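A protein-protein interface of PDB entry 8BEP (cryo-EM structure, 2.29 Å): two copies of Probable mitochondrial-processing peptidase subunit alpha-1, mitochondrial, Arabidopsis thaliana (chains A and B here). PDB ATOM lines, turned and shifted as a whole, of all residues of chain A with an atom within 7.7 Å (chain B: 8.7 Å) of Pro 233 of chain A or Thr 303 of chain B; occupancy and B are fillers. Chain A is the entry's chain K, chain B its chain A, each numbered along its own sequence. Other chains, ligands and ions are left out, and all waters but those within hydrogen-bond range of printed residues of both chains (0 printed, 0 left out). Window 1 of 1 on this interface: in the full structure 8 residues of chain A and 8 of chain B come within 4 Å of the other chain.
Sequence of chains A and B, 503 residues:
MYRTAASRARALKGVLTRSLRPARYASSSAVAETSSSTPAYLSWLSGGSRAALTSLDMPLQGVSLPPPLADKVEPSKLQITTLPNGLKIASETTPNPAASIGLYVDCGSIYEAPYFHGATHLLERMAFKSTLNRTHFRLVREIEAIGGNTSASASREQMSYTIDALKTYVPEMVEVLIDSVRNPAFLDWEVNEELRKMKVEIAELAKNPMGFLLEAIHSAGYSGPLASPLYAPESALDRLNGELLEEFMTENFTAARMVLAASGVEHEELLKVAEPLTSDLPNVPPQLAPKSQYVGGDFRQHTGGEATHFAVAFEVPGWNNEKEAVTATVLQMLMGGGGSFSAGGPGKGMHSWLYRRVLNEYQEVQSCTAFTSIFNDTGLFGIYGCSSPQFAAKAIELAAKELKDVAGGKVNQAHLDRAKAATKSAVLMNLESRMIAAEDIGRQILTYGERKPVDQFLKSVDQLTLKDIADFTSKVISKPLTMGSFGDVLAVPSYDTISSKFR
The backbone NH (N) of Gly 305 of chain B lies close to the side-chain hydroxyl (OG) of Ser 235 of chain A (3.2 Å).
The backbone NH (N) of Gly 304 of chain B sits at hydrogen-bond distance from the backbone carbonyl oxygen (O) of Gly 487 of chain B.
O of Gly 487 of chain B lies within hydrogen-bond range of N of Thr 303 of chain B, at 2.7 Å.
Among the printed residues, pairs that only touch across the chains: Ser 235 of chain A with Gly 304 of chain B (3.4 Å), Ser 235 of chain A with Thr 303 of chain B (3.4 Å), Pro 233 of chain A with His 302 of chain B (3.5 Å), Pro 233 of chain A with Thr 303 of chain B (3.5 Å) and Pro 229 of chain A with Leu 490 of chain B (3.9 Å).
Of chain B, only His 302 (3.5 Å) and Thr 303 (3.5 Å) come within 4 Å of Pro 233 of chain A.
Thr 303 of chain B touches two residues of chain A.
No residue of chain B comes within 4 Å of Ala 232 of chain A.
Of the printed residues of chain A, His 302 of chain B touches Pro 233.
Printed residues of chain B within 4 Å of Pro 229 of chain A: Leu 490 (3.9 Å).
Of the printed residues of chain A, Gly 305 of chain B touches Ser 235 (3.2 Å).
Of the printed residues of chain A, Leu 490 of chain B touches Pro 229.
Of the 17 printed residues of chain B, 5 touch a printed residue of chain A.
Hydrophobic or aromatic side chains of chain B that line the printed part of chain A: His 302 and Leu 490.
Printed residues of chain A that touch a printed residue of chain B: Pro 229, Pro 233 and Ser 235.
Hydrophobic or aromatic side chains of chain A that line the printed part of chain B: Pro 229 and Pro 233.
No position is printed for both chains.
Of the 6 pairs that touch across the chains among the printed residues, none has its exchanged pair printed and touching as well.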
ATOM      1  N   HIS A 117      12.435 -11.871  -9.249  1.00  0.00           N
ATOM      2  CA  HIS A 117      13.571 -11.905  -8.334  1.00  0.00           C
ATOM      3  C   HIS A 117      14.735 -12.668  -8.956  1.00  0.00           C
ATOM      4  O   HIS A 117      14.616 -13.855  -9.272  1.00  0.00           O
ATOM      5  CB  HIS A 117      13.159 -12.532  -7.003  1.00  0.00           C
ATOM      6  CG  HIS A 117      12.508 -11.565  -6.066  1.00  0.00           C
ATOM      7  ND1 HIS A 117      11.472 -11.918  -5.230  1.00  0.00           N
ATOM      8  CD2 HIS A 117      12.727 -10.245  -5.856  1.00  0.00           C
ATOM      9  CE1 HIS A 117      11.092 -10.863  -4.535  1.00  0.00           C
ATOM     10  NE2 HIS A 117      11.836  -9.834  -4.896  1.00  0.00           N
ATOM     11  N   GLY A 118      15.865 -11.982  -9.116  1.00  0.00           N
ATOM     12  CA  GLY A 118      17.023 -12.529  -9.786  1.00  0.00           C
ATOM     13  C   GLY A 118      17.174 -12.123 -11.232  1.00  0.00           C
ATOM     14  O   GLY A 118      18.157 -12.520 -11.867  1.00  0.00           O
ATOM     15  N   MET A 198      25.358 -19.212 -13.027  1.00  0.00           N
ATOM     16  CA  MET A 198      24.896 -18.416 -11.897  1.00  0.00           C
ATOM     17  C   MET A 198      24.835 -19.250 -10.627  1.00  0.00           C
ATOM     18  O   MET A 198      25.101 -18.746  -9.531  1.00  0.00           O
ATOM     19  CB  MET A 198      23.525 -17.819 -12.211  1.00  0.00           C
ATOM     20  CG  MET A 198      23.538 -16.342 -12.525  1.00  0.00           C
ATOM     21  SD  MET A 198      21.929 -15.729 -13.050  1.00  0.00           S
ATOM     22  CE  MET A 198      21.074 -15.603 -11.487  1.00  0.00           C
ATOM     23  N   LYS A 199      24.456 -20.525 -10.752  1.00  0.00           N
ATOM     24  CA  LYS A 199      24.430 -21.406  -9.586  1.00  0.00           C
ATOM     25  C   LYS A 199      25.792 -21.448  -8.901  1.00  0.00           C
ATOM     26  O   LYS A 199      25.902 -21.241  -7.685  1.00  0.00           O
ATOM     27  CB  LYS A 199      24.011 -22.819  -9.992  1.00  0.00           C
ATOM     28  CG  LYS A 199      22.649 -22.934 -10.639  1.00  0.00           C
ATOM     29  CD  LYS A 199      21.534 -22.608  -9.675  1.00  0.00           C
ATOM     30  CE  LYS A 199      20.209 -22.525 -10.405  1.00  0.00           C
ATOM     31  NZ  LYS A 199      20.385 -22.540 -11.884  1.00  0.00           N
ATOM     32  N   ILE A 202      26.781 -18.115  -7.273  1.00  0.00           N
ATOM     33  CA  ILE A 202      26.118 -17.956  -5.983  1.00  0.00           C
ATOM     34  C   ILE A 202      26.791 -18.822  -4.927  1.00  0.00           C
ATOM     35  O   ILE A 202      27.025 -18.379  -3.796  1.00  0.00           O
ATOM     36  CB  ILE A 202      24.621 -18.289  -6.115  1.00  0.00           C
ATOM     37  CG1 ILE A 202      23.860 -17.110  -6.714  1.00  0.00           C
ATOM     38  CG2 ILE A 202      24.037 -18.690  -4.769  1.00  0.00           C
ATOM     39  CD1 ILE A 202      23.482 -16.055  -5.709  1.00  0.00           C
ATOM     40  N   PRO A 229      17.406  -8.891  -2.772  1.00  0.00           N
ATOM     41  CA  PRO A 229      18.796  -9.274  -3.037  1.00  0.00           C
ATOM     42  C   PRO A 229      19.196  -9.010  -4.481  1.00  0.00           C
ATOM     43  O   PRO A 229      18.414  -9.217  -5.411  1.00  0.00           O
ATOM     44  CB  PRO A 229      18.818 -10.773  -2.716  1.00  0.00           C
ATOM     45  CG  PRO A 229      17.388 -11.201  -2.714  1.00  0.00           C
ATOM     46  CD  PRO A 229      16.597 -10.018  -2.285  1.00  0.00           C
ATOM     47  N   LEU A 230      20.433  -8.542  -4.659  1.00  0.00           N
ATOM     48  CA  LEU A 230      21.048  -8.564  -5.979  1.00  0.00           C
ATOM     49  C   LEU A 230      21.397  -9.992  -6.380  1.00  0.00           C
ATOM     50  O   LEU A 230      21.308 -10.357  -7.557  1.00  0.00           O
ATOM     51  CB  LEU A 230      22.292  -7.676  -5.987  1.00  0.00           C
ATOM     52  CG  LEU A 230      22.780  -7.035  -7.282  1.00  0.00           C
ATOM     53  CD1 LEU A 230      21.620  -6.523  -8.122  1.00  0.00           C
ATOM     54  CD2 LEU A 230      23.740  -5.908  -6.945  1.00  0.00           C
ATOM     55  N   TYR A 231      21.792 -10.812  -5.408  1.00  0.00           N
ATOM     56  CA  TYR A 231      22.062 -12.231  -5.609  1.00  0.00           C
ATOM     57  C   TYR A 231      20.828 -13.014  -5.175  1.00  0.00           C
ATOM     58  O   TYR A 231      20.556 -13.139  -3.976  1.00  0.00           O
ATOM     59  CB  TYR A 231      23.287 -12.669  -4.810  1.00  0.00           C
ATOM     60  CG  TYR A 231      24.607 -12.161  -5.336  1.00  0.00           C
ATOM     61  CD1 TYR A 231      25.018 -10.860  -5.095  1.00  0.00           C
ATOM     62  CD2 TYR A 231      25.454 -12.993  -6.055  1.00  0.00           C
ATOM     63  CE1 TYR A 231      26.222 -10.397  -5.565  1.00  0.00           C
ATOM     64  CE2 TYR A 231      26.664 -12.537  -6.529  1.00  0.00           C
ATOM     65  CZ  TYR A 231      27.043 -11.238  -6.281  1.00  0.00           C
ATOM     66  OH  TYR A 231      28.251 -10.775  -6.754  1.00  0.00           O
ATOM     67  N   ALA A 232      20.089 -13.544  -6.140  1.00  0.00           N
ATOM     68  CA  ALA A 232      18.866 -14.259  -5.819  1.00  0.00           C
ATOM     69  C   ALA A 232      19.174 -15.652  -5.275  1.00  0.00           C
ATOM     70  O   ALA A 232      20.212 -16.235  -5.595  1.00  0.00           O
ATOM     71  CB  ALA A 232      17.980 -14.377  -7.052  1.00  0.00           C
ATOM     72  N   PRO A 233      18.285 -16.207  -4.455  1.00  0.00           N
ATOM     73  CA  PRO A 233      18.505 -17.560  -3.936  1.00  0.00           C
ATOM     74  C   PRO A 233      18.300 -18.608  -5.017  1.00  0.00           C
ATOM     75  O   PRO A 233      17.685 -18.361  -6.057  1.00  0.00           O
ATOM     76  CB  PRO A 233      17.455 -17.692  -2.833  1.00  0.00           C
ATOM     77  CG  PRO A 233      16.370 -16.773  -3.245  1.00  0.00           C
ATOM     78  CD  PRO A 233      17.006 -15.639  -3.993  1.00  0.00           C
ATOM     79  N   GLU A 234      18.817 -19.807  -4.750  1.00  0.00           N
ATOM     80  CA  GLU A 234      18.738 -20.883  -5.728  1.00  0.00           C
ATOM     81  C   GLU A 234      17.377 -21.562  -5.664  1.00  0.00           C
ATOM     82  O   GLU A 234      17.279 -22.793  -5.648  1.00  0.00           O
ATOM     83  CB  GLU A 234      19.860 -21.901  -5.496  1.00  0.00           C
ATOM     84  CG  GLU A 234      19.936 -22.456  -4.074  1.00  0.00           C
ATOM     85  CD  GLU A 234      20.683 -21.544  -3.119  1.00  0.00           C
ATOM     86  OE1 GLU A 234      20.173 -20.443  -2.824  1.00  0.00           O
ATOM     87  OE2 GLU A 234      21.779 -21.929  -2.660  1.00  0.00           O
ATOM     88  N   SER A 235      16.332 -20.764  -5.631  1.00  0.00           N
ATOM     89  CA  SER A 235      14.944 -21.159  -5.813  1.00  0.00           C
ATOM     90  C   SER A 235      14.236 -20.277  -6.826  1.00  0.00           C
ATOM     91  O   SER A 235      13.409 -20.771  -7.596  1.00  0.00           O
ATOM     92  CB  SER A 235      14.198 -21.124  -4.471  1.00  0.00           C
ATOM     93  OG  SER A 235      12.813 -20.910  -4.670  1.00  0.00           O
ATOM     94  N   ALA A 236      14.548 -18.981  -6.847  1.00  0.00           N
ATOM     95  CA  ALA A 236      14.066 -18.103  -7.901  1.00  0.00           C
ATOM     96  C   ALA A 236      14.783 -18.343  -9.220  1.00  0.00           C
ATOM     97  O   ALA A 236      14.320 -17.861 -10.257  1.00  0.00           O
ATOM     98  CB  ALA A 236      14.225 -16.640  -7.483  1.00  0.00           C
ATOM     99  N   LEU A 237      15.907 -19.063  -9.197  1.00  0.00           N
ATOM    100  CA  LEU A 237      16.640 -19.357 -10.423  1.00  0.00           C
ATOM    101  C   LEU A 237      15.981 -20.464 -11.231  1.00  0.00           C
ATOM    102  O   LEU A 237      15.975 -20.403 -12.465  1.00  0.00           O
ATOM    103  CB  LEU A 237      18.084 -19.738 -10.093  1.00  0.00           C
ATOM    104  CG  LEU A 237      18.849 -18.750  -9.210  1.00  0.00           C
ATOM    105  CD1 LEU A 237      20.333 -19.073  -9.197  1.00  0.00           C
ATOM    106  CD2 LEU A 237      18.606 -17.324  -9.671  1.00  0.00           C
ATOM    107  N   ASP A 238      15.422 -21.475 -10.561  1.00  0.00           N
ATOM    108  CA  ASP A 238      14.717 -22.546 -11.253  1.00  0.00           C
ATOM    109  C   ASP A 238      13.485 -22.047 -11.991  1.00  0.00           C
ATOM    110  O   ASP A 238      12.967 -22.762 -12.856  1.00  0.00           O
ATOM    111  CB  ASP A 238      14.316 -23.636 -10.257  1.00  0.00           C
ATOM    112  CG  ASP A 238      15.504 -24.437  -9.756  1.00  0.00           C
ATOM    113  OD1 ASP A 238      16.616 -23.873  -9.683  1.00  0.00           O
ATOM    114  OD2 ASP A 238      15.324 -25.628  -9.430  1.00  0.00           O
ATOM    115  N   LEU A 240      13.460 -18.716 -13.369  1.00  0.00           N
ATOM    116  CA  LEU A 240      13.876 -17.727 -14.352  1.00  0.00           C
ATOM    117  C   LEU A 240      13.995 -18.366 -15.732  1.00  0.00           C
ATOM    118  O   LEU A 240      14.480 -19.493 -15.869  1.00  0.00           O
ATOM    119  CB  LEU A 240      15.204 -17.101 -13.928  1.00  0.00           C
ATOM    120  CG  LEU A 240      15.111 -15.894 -12.988  1.00  0.00           C
ATOM    121  CD1 LEU A 240      16.490 -15.477 -12.507  1.00  0.00           C
ATOM    122  CD2 LEU A 240      14.413 -14.731 -13.670  1.00  0.00           C
ATOM    123  N   ALA B 206      15.743 -29.734   7.175  1.00  0.00           N
ATOM    124  CA  ALA B 206      14.944 -28.710   6.515  1.00  0.00           C
ATOM    125  C   ALA B 206      13.595 -29.240   6.050  1.00  0.00           C
ATOM    126  O   ALA B 206      12.721 -28.447   5.687  1.00  0.00           O
ATOM    127  CB  ALA B 206      15.716 -28.129   5.330  1.00  0.00           C
ATOM    128  N   PHE B 212      12.664 -27.694  12.647  1.00  0.00           N
ATOM    129  CA  PHE B 212      13.685 -26.719  12.278  1.00  0.00           C
ATOM    130  C   PHE B 212      13.448 -25.388  12.978  1.00  0.00           C
ATOM    131  O   PHE B 212      14.366 -24.813  13.573  1.00  0.00           O
ATOM    132  CB  PHE B 212      13.701 -26.539  10.761  1.00  0.00           C
ATOM    133  CG  PHE B 212      14.881 -25.771  10.255  1.00  0.00           C
ATOM    134  CD1 PHE B 212      16.090 -26.401  10.027  1.00  0.00           C
ATOM    135  CD2 PHE B 212      14.782 -24.414  10.005  1.00  0.00           C
ATOM    136  CE1 PHE B 212      17.176 -25.691   9.563  1.00  0.00           C
ATOM    137  CE2 PHE B 212      15.862 -23.703   9.543  1.00  0.00           C
ATOM    138  CZ  PHE B 212      17.061 -24.342   9.320  1.00  0.00           C
ATOM    139  N   PHE B 299      15.086 -15.277  13.902  1.00  0.00           N
ATOM    140  CA  PHE B 299      15.763 -16.235  13.041  1.00  0.00           C
ATOM    141  C   PHE B 299      15.188 -16.117  11.642  1.00  0.00           C
ATOM    142  O   PHE B 299      13.969 -16.201  11.463  1.00  0.00           O
ATOM    143  CB  PHE B 299      15.591 -17.667  13.540  1.00  0.00           C
ATOM    144  CG  PHE B 299      15.987 -18.701  12.531  1.00  0.00           C
ATOM    145  CD1 PHE B 299      17.319 -18.936  12.252  1.00  0.00           C
ATOM    146  CD2 PHE B 299      15.024 -19.407  11.829  1.00  0.00           C
ATOM    147  CE1 PHE B 299      17.685 -19.880  11.320  1.00  0.00           C
ATOM    148  CE2 PHE B 299      15.383 -20.348  10.898  1.00  0.00           C
ATOM    149  CZ  PHE B 299      16.718 -20.586  10.641  1.00  0.00           C
ATOM    150  N   ARG B 300      16.059 -15.952  10.649  1.00  0.00           N
ATOM    151  CA  ARG B 300      15.599 -15.688   9.289  1.00  0.00           C
ATOM    152  C   ARG B 300      16.542 -16.337   8.295  1.00  0.00           C
ATOM    153  O   ARG B 300      17.709 -15.946   8.192  1.00  0.00           O
ATOM    154  CB  ARG B 300      15.501 -14.187   9.035  1.00  0.00           C
ATOM    155  CG  ARG B 300      14.284 -13.591   9.672  1.00  0.00           C
ATOM    156  CD  ARG B 300      13.980 -12.193   9.230  1.00  0.00           C
ATOM    157  NE  ARG B 300      12.763 -11.759   9.900  1.00  0.00           N
ATOM    158  CZ  ARG B 300      12.249 -10.542   9.831  1.00  0.00           C
ATOM    159  NH1 ARG B 300      12.830  -9.583   9.128  1.00  0.00           N
ATOM    160  NH2 ARG B 300      11.123 -10.282  10.485  1.00  0.00           N
ATOM    161  N   GLN B 301      16.035 -17.324   7.570  1.00  0.00           N
ATOM    162  CA  GLN B 301      16.737 -17.918   6.443  1.00  0.00           C
ATOM    163  C   GLN B 301      15.853 -17.759   5.216  1.00  0.00           C
ATOM    164  O   GLN B 301      14.930 -18.551   5.003  1.00  0.00           O
ATOM    165  CB  GLN B 301      17.066 -19.385   6.702  1.00  0.00           C
ATOM    166  CG  GLN B 301      18.499 -19.627   7.126  1.00  0.00           C
ATOM    167  CD  GLN B 301      18.817 -21.100   7.257  1.00  0.00           C
ATOM    168  OE1 GLN B 301      18.275 -21.929   6.526  1.00  0.00           O
ATOM    169  NE2 GLN B 301      19.699 -21.435   8.191  1.00  0.00           N
ATOM    170  N   HIS B 302      16.133 -16.736   4.417  1.00  0.00           N
ATOM    171  CA  HIS B 302      15.392 -16.496   3.184  1.00  0.00           C
ATOM    172  C   HIS B 302      15.850 -17.511   2.148  1.00  0.00           C
ATOM    173  O   HIS B 302      16.911 -17.363   1.535  1.00  0.00           O
ATOM    174  CB  HIS B 302      15.599 -15.068   2.696  1.00  0.00           C
ATOM    175  CG  HIS B 302      15.317 -14.885   1.239  1.00  0.00           C
ATOM    176  ND1 HIS B 302      16.260 -14.409   0.353  1.00  0.00           N
ATOM    177  CD2 HIS B 302      14.205 -15.132   0.508  1.00  0.00           C
ATOM    178  CE1 HIS B 302      15.737 -14.360  -0.858  1.00  0.00           C
ATOM    179  NE2 HIS B 302      14.492 -14.796  -0.793  1.00  0.00           N
ATOM    180  N   THR B 303      15.056 -18.562   1.967  1.00  0.00           N
ATOM    181  CA  THR B 303      15.328 -19.551   0.937  1.00  0.00           C
ATOM    182  C   THR B 303      14.561 -19.280  -0.347  1.00  0.00           C
ATOM    183  O   THR B 303      14.961 -19.774  -1.408  1.00  0.00           O
ATOM    184  CB  THR B 303      14.986 -20.953   1.444  1.00  0.00           C
ATOM    185  OG1 THR B 303      15.797 -21.261   2.585  1.00  0.00           O
ATOM    186  CG2 THR B 303      15.243 -21.986   0.359  1.00  0.00           C
ATOM    187  N   GLY B 304      13.479 -18.511  -0.275  1.00  0.00           N
ATOM    188  CA  GLY B 304      12.688 -18.201  -1.445  1.00  0.00           C
ATOM    189  C   GLY B 304      11.773 -19.343  -1.835  1.00  0.00           C
ATOM    190  O   GLY B 304      11.799 -20.440  -1.271  1.00  0.00           O
ATOM    191  N   GLY B 305      10.939 -19.068  -2.832  1.00  0.00           N
ATOM    192  CA  GLY B 305      10.038 -20.076  -3.353  1.00  0.00           C
ATOM    193  C   GLY B 305       8.608 -19.930  -2.882  1.00  0.00           C
ATOM    194  O   GLY B 305       7.885 -19.035  -3.328  1.00  0.00           O
ATOM    195  N   GLU B 306       8.190 -20.806  -1.974  1.00  0.00           N
ATOM    196  CA  GLU B 306       6.799 -20.878  -1.551  1.00  0.00           C
ATOM    197  C   GLU B 306       6.751 -21.476  -0.153  1.00  0.00           C
ATOM    198  O   GLU B 306       7.777 -21.872   0.409  1.00  0.00           O
ATOM    199  CB  GLU B 306       5.975 -21.709  -2.540  1.00  0.00           C
ATOM    200  CG  GLU B 306       6.021 -23.223  -2.303  1.00  0.00           C
ATOM    201  CD  GLU B 306       7.362 -23.872  -2.640  1.00  0.00           C
ATOM    202  OE1 GLU B 306       8.412 -23.196  -2.585  1.00  0.00           O
ATOM    203  OE2 GLU B 306       7.362 -25.079  -2.959  1.00  0.00           O
ATOM    204  N   ALA B 307       5.541 -21.533   0.408  1.00  0.00           N
ATOM    205  CA  ALA B 307       5.263 -22.242   1.655  1.00  0.00           C
ATOM    206  C   ALA B 307       6.127 -21.704   2.800  1.00  0.00           C
ATOM    207  O   ALA B 307       7.013 -22.380   3.329  1.00  0.00           O
ATOM    208  CB  ALA B 307       5.455 -23.752   1.477  1.00  0.00           C
ATOM    209  N   SER B 485      11.240 -17.406  11.307  1.00  0.00           N
ATOM    210  CA  SER B 485      10.584 -17.664  10.035  1.00  0.00           C
ATOM    211  C   SER B 485      11.531 -18.440   9.133  1.00  0.00           C
ATOM    212  O   SER B 485      12.754 -18.338   9.257  1.00  0.00           O
ATOM    213  CB  SER B 485      10.140 -16.363   9.350  1.00  0.00           C
ATOM    214  OG  SER B 485      11.021 -15.297   9.654  1.00  0.00           O
ATOM    215  N   PHE B 486      10.952 -19.217   8.221  1.00  0.00           N
ATOM    216  CA  PHE B 486      11.726 -20.134   7.391  1.00  0.00           C
ATOM    217  C   PHE B 486      10.992 -20.333   6.074  1.00  0.00           C
ATOM    218  O   PHE B 486       9.843 -20.787   6.062  1.00  0.00           O
ATOM    219  CB  PHE B 486      11.934 -21.469   8.115  1.00  0.00           C
ATOM    220  CG  PHE B 486      12.374 -22.593   7.222  1.00  0.00           C
ATOM    221  CD1 PHE B 486      13.447 -22.439   6.361  1.00  0.00           C
ATOM    222  CD2 PHE B 486      11.718 -23.809   7.253  1.00  0.00           C
ATOM    223  CE1 PHE B 486      13.851 -23.477   5.541  1.00  0.00           C
ATOM    224  CE2 PHE B 486      12.116 -24.852   6.436  1.00  0.00           C
ATOM    225  CZ  PHE B 486      13.184 -24.685   5.579  1.00  0.00           C
ATOM    226  N   GLY B 487      11.657 -20.003   4.974  1.00  0.00           N
ATOM    227  CA  GLY B 487      11.049 -20.084   3.661  1.00  0.00           C
ATOM    228  C   GLY B 487      11.283 -18.818   2.865  1.00  0.00           C
ATOM    229  O   GLY B 487      12.430 -18.433   2.621  1.00  0.00           O
ATOM    230  N   ASP B 488      10.204 -18.162   2.452  1.00  0.00           N
ATOM    231  CA  ASP B 488      10.279 -16.852   1.815  1.00  0.00           C
ATOM    232  C   ASP B 488       9.995 -15.815   2.893  1.00  0.00           C
ATOM    233  O   ASP B 488       8.850 -15.641   3.316  1.00  0.00           O
ATOM    234  CB  ASP B 488       9.299 -16.743   0.652  1.00  0.00           C
ATOM    235  CG  ASP B 488       9.364 -15.394  -0.035  1.00  0.00           C
ATOM    236  OD1 ASP B 488      10.414 -15.080  -0.634  1.00  0.00           O
ATOM    237  OD2 ASP B 488       8.368 -14.644   0.030  1.00  0.00           O
ATOM    238  N   VAL B 489      11.047 -15.126   3.338  1.00  0.00           N
ATOM    239  CA  VAL B 489      10.935 -14.187   4.449  1.00  0.00           C
ATOM    240  C   VAL B 489      10.864 -12.737   3.974  1.00  0.00           C
ATOM    241  O   VAL B 489      10.656 -11.832   4.800  1.00  0.00           O
ATOM    242  CB  VAL B 489      12.104 -14.396   5.443  1.00  0.00           C
ATOM    243  CG1 VAL B 489      11.915 -13.598   6.726  1.00  0.00           C
ATOM    244  CG2 VAL B 489      12.261 -15.875   5.764  1.00  0.00           C
ATOM    245  N   LEU B 490      10.985 -12.488   2.667  1.00  0.00           N
ATOM    246  CA  LEU B 490      10.993 -11.114   2.171  1.00  0.00           C
ATOM    247  C   LEU B 490       9.700 -10.389   2.512  1.00  0.00           C
ATOM    248  O   LEU B 490       9.723  -9.234   2.950  1.00  0.00           O
ATOM    249  CB  LEU B 490      11.217 -11.098   0.659  1.00  0.00           C
ATOM    250  CG  LEU B 490      12.630 -11.352   0.138  1.00  0.00           C
ATOM    251  CD1 LEU B 490      12.570 -12.255  -1.076  1.00  0.00           C
ATOM    252  CD2 LEU B 490      13.324 -10.043  -0.196  1.00  0.00           C
